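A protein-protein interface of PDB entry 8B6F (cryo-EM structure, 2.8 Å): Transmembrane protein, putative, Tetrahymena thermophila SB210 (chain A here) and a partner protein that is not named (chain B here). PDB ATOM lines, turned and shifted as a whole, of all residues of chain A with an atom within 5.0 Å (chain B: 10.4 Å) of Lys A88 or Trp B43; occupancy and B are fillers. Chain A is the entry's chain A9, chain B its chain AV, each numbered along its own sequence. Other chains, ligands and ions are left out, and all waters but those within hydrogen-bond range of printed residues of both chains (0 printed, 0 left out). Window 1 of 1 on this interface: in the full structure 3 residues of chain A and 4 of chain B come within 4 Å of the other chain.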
ATOM      1  N   SER A  84       9.338   5.130 -10.327  1.00  0.00           N
ATOM      2  CA  SER A  84       9.582   4.695 -11.698  1.00  0.00           C
ATOM      3  C   SER A  84       9.683   5.884 -12.644  1.00  0.00           C
ATOM      4  O   SER A  84      10.544   5.909 -13.530  1.00  0.00           O
ATOM      5  CB  SER A  84       8.472   3.749 -12.153  1.00  0.00           C
ATOM      6  OG  SER A  84       8.403   2.605 -11.323  1.00  0.00           O
ATOM      7  N   ILE A  85       8.819   6.883 -12.466  1.00  0.00           N
ATOM      8  CA  ILE A  85       8.848   8.051 -13.343  1.00  0.00           C
ATOM      9  C   ILE A  85      10.157   8.810 -13.170  1.00  0.00           C
ATOM     10  O   ILE A  85      10.750   9.282 -14.147  1.00  0.00           O
ATOM     11  CB  ILE A  85       7.624   8.949 -13.081  1.00  0.00           C
ATOM     12  CG1 ILE A  85       7.562  10.064 -14.127  1.00  0.00           C
ATOM     13  CG2 ILE A  85       7.668   9.533 -11.676  1.00  0.00           C
ATOM     14  CD1 ILE A  85       6.293  10.888 -14.075  1.00  0.00           C
ATOM     15  N   VAL A  86      10.625   8.947 -11.930  1.00  0.00           N
ATOM     16  CA  VAL A  86      11.897   9.623 -11.693  1.00  0.00           C
ATOM     17  C   VAL A  86      13.032   8.852 -12.350  1.00  0.00           C
ATOM     18  O   VAL A  86      13.929   9.442 -12.963  1.00  0.00           O
ATOM     19  CB  VAL A  86      12.130   9.803 -10.182  1.00  0.00           C
ATOM     20  CG1 VAL A  86      13.495  10.423  -9.916  1.00  0.00           C
ATOM     21  CG2 VAL A  86      11.030  10.660  -9.579  1.00  0.00           C
ATOM     22  N   LEU A  87      13.018   7.524 -12.225  1.00  0.00           N
ATOM     23  CA  LEU A  87      14.051   6.713 -12.864  1.00  0.00           C
ATOM     24  C   LEU A  87      14.027   6.884 -14.376  1.00  0.00           C
ATOM     25  O   LEU A  87      15.080   7.002 -15.012  1.00  0.00           O
ATOM     26  CB  LEU A  87      13.874   5.243 -12.486  1.00  0.00           C
ATOM     27  CG  LEU A  87      14.153   4.880 -11.025  1.00  0.00           C
ATOM     28  CD1 LEU A  87      13.788   3.432 -10.761  1.00  0.00           C
ATOM     29  CD2 LEU A  87      15.611   5.133 -10.669  1.00  0.00           C
ATOM     30  N   LYS A  88      12.836   6.886 -14.973  1.00  0.00           N
ATOM     31  CA  LYS A  88      12.741   7.071 -16.418  1.00  0.00           C
ATOM     32  C   LYS A  88      13.268   8.439 -16.832  1.00  0.00           C
ATOM     33  O   LYS A  88      13.980   8.560 -17.835  1.00  0.00           O
ATOM     34  CB  LYS A  88      11.293   6.896 -16.872  1.00  0.00           C
ATOM     35  CG  LYS A  88      10.761   5.483 -16.711  1.00  0.00           C
ATOM     36  CD  LYS A  88       9.311   5.394 -17.147  1.00  0.00           C
ATOM     37  CE  LYS A  88       8.777   3.978 -17.031  1.00  0.00           C
ATOM     38  NZ  LYS A  88       8.779   3.492 -15.629  1.00  0.00           N
ATOM     39  N   LYS A  89      12.921   9.484 -16.079  1.00  0.00           N
ATOM     40  CA  LYS A  89      13.386  10.824 -16.419  1.00  0.00           C
ATOM     41  C   LYS A  89      14.904  10.931 -16.334  1.00  0.00           C
ATOM     42  O   LYS A  89      15.539  11.531 -17.208  1.00  0.00           O
ATOM     43  CB  LYS A  89      12.731  11.854 -15.499  1.00  0.00           C
ATOM     44  CG  LYS A  89      11.260  12.101 -15.783  1.00  0.00           C
ATOM     45  CD  LYS A  89      11.062  12.814 -17.111  1.00  0.00           C
ATOM     46  CE  LYS A  89       9.598  13.142 -17.340  1.00  0.00           C
ATOM     47  NZ  LYS A  89       9.379  13.801 -18.654  1.00  0.00           N
ATOM     48  N   MET A  90      15.507  10.364 -15.287  1.00  0.00           N
ATOM     49  CA  MET A  90      16.957  10.457 -15.155  1.00  0.00           C
ATOM     50  C   MET A  90      17.669   9.608 -16.199  1.00  0.00           C
ATOM     51  O   MET A  90      18.738   9.996 -16.678  1.00  0.00           O
ATOM     52  CB  MET A  90      17.393  10.066 -13.740  1.00  0.00           C
ATOM     53  CG  MET A  90      16.977   8.687 -13.294  1.00  0.00           C
ATOM     54  SD  MET A  90      16.999   8.523 -11.496  1.00  0.00           S
ATOM     55  CE  MET A  90      18.709   8.898 -11.133  1.00  0.00           C
ATOM     56  N   PHE A  91      17.100   8.461 -16.573  1.00  0.00           N
ATOM     57  CA  PHE A  91      17.672   7.684 -17.670  1.00  0.00           C
ATOM     58  C   PHE A  91      17.583   8.450 -18.981  1.00  0.00           C
ATOM     59  O   PHE A  91      18.513   8.417 -19.793  1.00  0.00           O
ATOM     60  CB  PHE A  91      16.977   6.327 -17.792  1.00  0.00           C
ATOM     61  CG  PHE A  91      17.091   5.469 -16.561  1.00  0.00           C
ATOM     62  CD1 PHE A  91      18.070   5.711 -15.608  1.00  0.00           C
ATOM     63  CD2 PHE A  91      16.219   4.414 -16.362  1.00  0.00           C
ATOM     64  CE1 PHE A  91      18.170   4.919 -14.483  1.00  0.00           C
ATOM     65  CE2 PHE A  91      16.315   3.620 -15.238  1.00  0.00           C
ATOM     66  CZ  PHE A  91      17.292   3.873 -14.298  1.00  0.00           C
ATOM     67  N   ARG A  92      16.471   9.151 -19.203  1.00  0.00           N
ATOM     68  CA  ARG A  92      16.356  10.001 -20.383  1.00  0.00           C
ATOM     69  C   ARG A  92      17.413  11.094 -20.368  1.00  0.00           C
ATOM     70  O   ARG A  92      17.979  11.436 -21.412  1.00  0.00           O
ATOM     71  CB  ARG A  92      14.957  10.608 -20.466  1.00  0.00           C
ATOM     72  CG  ARG A  92      14.829  11.691 -21.524  1.00  0.00           C
ATOM     73  CD  ARG A  92      13.377  12.060 -21.763  1.00  0.00           C
ATOM     74  NE  ARG A  92      13.239  13.148 -22.724  1.00  0.00           N
ATOM     75  CZ  ARG A  92      13.250  14.436 -22.411  1.00  0.00           C
ATOM     76  NH1 ARG A  92      13.394  14.845 -21.162  1.00  0.00           N
ATOM     77  NH2 ARG A  92      13.110  15.339 -23.378  1.00  0.00           N
ATOM     78  N   ARG A  95      20.591   9.589 -21.551  1.00  0.00           N
ATOM     79  CA  ARG A  95      20.597   9.416 -22.999  1.00  0.00           C
ATOM     80  C   ARG A  95      20.854  10.739 -23.709  1.00  0.00           C
ATOM     81  O   ARG A  95      21.590  10.787 -24.701  1.00  0.00           O
ATOM     82  CB  ARG A  95      19.269   8.817 -23.464  1.00  0.00           C
ATOM     83  CG  ARG A  95      18.980   7.430 -22.913  1.00  0.00           C
ATOM     84  CD  ARG A  95      17.897   6.739 -23.720  1.00  0.00           C
ATOM     85  NE  ARG A  95      16.763   7.616 -23.982  1.00  0.00           N
ATOM     86  CZ  ARG A  95      15.712   7.755 -23.184  1.00  0.00           C
ATOM     87  NH1 ARG A  95      15.616   7.093 -22.043  1.00  0.00           N
ATOM     88  NH2 ARG A  95      14.731   8.578 -23.541  1.00  0.00           N
ATOM     89  N   ASN B  39       6.621  -4.436  -0.898  1.00  0.00           N
ATOM     90  CA  ASN B  39       6.927  -3.438  -1.913  1.00  0.00           C
ATOM     91  C   ASN B  39       6.085  -3.682  -3.158  1.00  0.00           C
ATOM     92  O   ASN B  39       5.982  -4.813  -3.640  1.00  0.00           O
ATOM     93  CB  ASN B  39       8.414  -3.486  -2.258  1.00  0.00           C
ATOM     94  CG  ASN B  39       8.819  -2.406  -3.236  1.00  0.00           C
ATOM     95  OD1 ASN B  39       8.157  -1.376  -3.349  1.00  0.00           O
ATOM     96  ND2 ASN B  39       9.910  -2.639  -3.953  1.00  0.00           N
ATOM     97  N   SER B  40       5.481  -2.612  -3.680  1.00  0.00           N
ATOM     98  CA  SER B  40       4.591  -2.697  -4.833  1.00  0.00           C
ATOM     99  C   SER B  40       5.063  -1.827  -5.993  1.00  0.00           C
ATOM    100  O   SER B  40       4.271  -1.504  -6.881  1.00  0.00           O
ATOM    101  CB  SER B  40       3.165  -2.312  -4.433  1.00  0.00           C
ATOM    102  OG  SER B  40       3.113  -0.979  -3.957  1.00  0.00           O
ATOM    103  N   ALA B  41       6.336  -1.444  -6.006  1.00  0.00           N
ATOM    104  CA  ALA B  41       6.858  -0.584  -7.059  1.00  0.00           C
ATOM    105  C   ALA B  41       7.210  -1.415  -8.286  1.00  0.00           C
ATOM    106  O   ALA B  41       7.922  -2.418  -8.185  1.00  0.00           O
ATOM    107  CB  ALA B  41       8.087   0.175  -6.563  1.00  0.00           C
ATOM    108  N   THR B  42       6.713  -0.989  -9.445  1.00  0.00           N
ATOM    109  CA  THR B  42       6.951  -1.679 -10.704  1.00  0.00           C
ATOM    110  C   THR B  42       7.359  -0.674 -11.770  1.00  0.00           C
ATOM    111  O   THR B  42       6.937   0.484 -11.751  1.00  0.00           O
ATOM    112  CB  THR B  42       5.712  -2.450 -11.171  1.00  0.00           C
ATOM    113  OG1 THR B  42       4.618  -1.541 -11.349  1.00  0.00           O
ATOM    114  CG2 THR B  42       5.324  -3.507 -10.153  1.00  0.00           C
ATOM    115  N   TRP B  43       8.195  -1.135 -12.701  1.00  0.00           N
ATOM    116  CA  TRP B  43       8.681  -0.263 -13.765  1.00  0.00           C
ATOM    117  C   TRP B  43       7.554   0.177 -14.690  1.00  0.00           C
ATOM    118  O   TRP B  43       7.495   1.343 -15.096  1.00  0.00           O
ATOM    119  CB  TRP B  43       9.774  -0.978 -14.559  1.00  0.00           C
ATOM    120  CG  TRP B  43      10.258  -0.205 -15.741  1.00  0.00           C
ATOM    121  CD1 TRP B  43       9.820  -0.314 -17.026  1.00  0.00           C
ATOM    122  CD2 TRP B  43      11.279   0.801 -15.749  1.00  0.00           C
ATOM    123  NE1 TRP B  43      10.503   0.562 -17.835  1.00  0.00           N
ATOM    124  CE2 TRP B  43      11.405   1.258 -17.075  1.00  0.00           C
ATOM    125  CE3 TRP B  43      12.098   1.359 -14.762  1.00  0.00           C
ATOM    126  CZ2 TRP B  43      12.316   2.246 -17.439  1.00  0.00           C
ATOM    127  CZ3 TRP B  43      13.002   2.340 -15.125  1.00  0.00           C
ATOM    128  CH2 TRP B  43      13.104   2.773 -16.453  1.00  0.00           C
ATOM    129  N   ALA B  44       6.649  -0.740 -15.036  1.00  0.00           N
ATOM    130  CA  ALA B  44       5.654  -0.446 -16.060  1.00  0.00           C
ATOM    131  C   ALA B  44       4.732   0.692 -15.643  1.00  0.00           C
ATOM    132  O   ALA B  44       4.443   1.590 -16.441  1.00  0.00           O
ATOM    133  CB  ALA B  44       4.838  -1.701 -16.369  1.00  0.00           C
ATOM    134  N   HIS B  45       4.260   0.676 -14.400  1.00  0.00           N
ATOM    135  CA  HIS B  45       3.251   1.625 -13.939  1.00  0.00           C
ATOM    136  C   HIS B  45       3.937   2.883 -13.418  1.00  0.00           C
ATOM    137  O   HIS B  45       4.576   2.858 -12.362  1.00  0.00           O
ATOM    138  CB  HIS B  45       2.380   0.994 -12.857  1.00  0.00           C
ATOM    139  CG  HIS B  45       1.671  -0.246 -13.301  1.00  0.00           C
ATOM    140  ND1 HIS B  45       2.299  -1.469 -13.396  1.00  0.00           N
ATOM    141  CD2 HIS B  45       0.391  -0.450 -13.688  1.00  0.00           C
ATOM    142  CE1 HIS B  45       1.433  -2.374 -13.817  1.00  0.00           C
ATOM    143  NE2 HIS B  45       0.268  -1.782 -14.002  1.00  0.00           N
ATOM    144  N   ASN B  46       3.803   3.985 -14.160  1.00  0.00           N
ATOM    145  CA  ASN B  46       4.282   5.267 -13.655  1.00  0.00           C
ATOM    146  C   ASN B  46       3.508   5.683 -12.413  1.00  0.00           C
ATOM    147  O   ASN B  46       4.091   6.185 -11.446  1.00  0.00           O
ATOM    148  CB  ASN B  46       4.170   6.340 -14.737  1.00  0.00           C
ATOM    149  CG  ASN B  46       5.243   6.211 -15.797  1.00  0.00           C
ATOM    150  OD1 ASN B  46       6.337   5.721 -15.531  1.00  0.00           O
ATOM    151  ND2 ASN B  46       4.935   6.656 -17.008  1.00  0.00           N
ATOM    152  N   LEU B  47       2.191   5.484 -12.422  1.00  0.00           N
ATOM    153  CA  LEU B  47       1.380   5.697 -11.234  1.00  0.00           C
ATOM    154  C   LEU B  47       1.395   4.426 -10.396  1.00  0.00           C
ATOM    155  O   LEU B  47       0.903   3.390 -10.863  1.00  0.00           O
ATOM    156  CB  LEU B  47      -0.046   6.057 -11.616  1.00  0.00           C
ATOM    157  CG  LEU B  47      -0.962   6.518 -10.480  1.00  0.00           C
ATOM    158  CD1 LEU B  47      -0.508   7.856  -9.926  1.00  0.00           C
ATOM    159  CD2 LEU B  47      -2.401   6.603 -10.955  1.00  0.00           C
ATOM    160  N   PRO B  48       1.933   4.447  -9.176  1.00  0.00           N
ATOM    161  CA  PRO B  48       2.090   3.195  -8.428  1.00  0.00           C
ATOM    162  C   PRO B  48       0.753   2.543  -8.114  1.00  0.00           C
ATOM    163  O   PRO B  48      -0.265   3.212  -7.923  1.00  0.00           O
ATOM    164  CB  PRO B  48       2.814   3.633  -7.149  1.00  0.00           C
ATOM    165  CG  PRO B  48       2.484   5.066  -7.002  1.00  0.00           C
ATOM    166  CD  PRO B  48       2.389   5.608  -8.396  1.00  0.00           C
ATOM    167  N   LYS B  49       0.771   1.215  -8.062  1.00  0.00           N
ATOM    168  CA  LYS B  49      -0.415   0.442  -7.734  1.00  0.00           C
ATOM    169  C   LYS B  49      -0.697   0.501  -6.236  1.00  0.00           C
ATOM    170  O   LYS B  49       0.189   0.752  -5.416  1.00  0.00           O
ATOM    171  CB  LYS B  49      -0.243  -1.008  -8.181  1.00  0.00           C
ATOM    172  CG  LYS B  49      -0.157  -1.177  -9.690  1.00  0.00           C
ATOM    173  CD  LYS B  49       0.816  -2.279 -10.080  1.00  0.00           C
ATOM    174  CE  LYS B  49       0.409  -3.626  -9.505  1.00  0.00           C
ATOM    175  NZ  LYS B  49       1.345  -4.706  -9.932  1.00  0.00           N
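Among the printed residues, pairs that only touch across the chains: Ser A84 with Trp B43, Ser A84 with His B45 and Phe A91 with Trp B43.
Hydrophobic or aromatic side chains of chain B within 4 Å of the printed part of chain A: Trp B43.
Of the 10 printed residues of chain A, 3 touch a printed residue of chain B.
Hydrophobic or aromatic side chains of chain A that line the printed part of chain B: Phe A91.
The side-chain amino group (NZ) of Lys A88 is in hydrogen-bond range of the side-chain amide oxygen (OD1) of Asn B46 (3.3 Å).
The side-chain amino group (NZ) of Lys A88 is in hydrogen-bond range of the backbone carbonyl oxygen (O) of Trp B43 (2.6 Å).
O of Thr B42 lies within hydrogen-bond range of OG of Ser A84 (2.6 Å).
Of chain B, only Thr B42 (2.6 Å), Trp B43 (3.8 Å) and His B45 (3.97 Å) come within 4 Å of Ser A84.
Val A86 touches none of the printed residues of chain B.
Lys A88 touches just these residues of chain B: Trp B43 (2.6 Å) and Asn B46 (3.3 Å).
Printed residues of chain A within 4 Å of Thr B42: Ser A84.
Ala B44 touches none of the printed residues of chain A.
Of the printed residues of chain A, Asn B46 touches Lys A88.
The nearest printed residue of chain A that does not touch Trp B43 is Leu A87 (4.02 Å).
ND1 of His B45 is in hydrogen-bond range of OG1 of Thr B42, 3.1 Å away.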
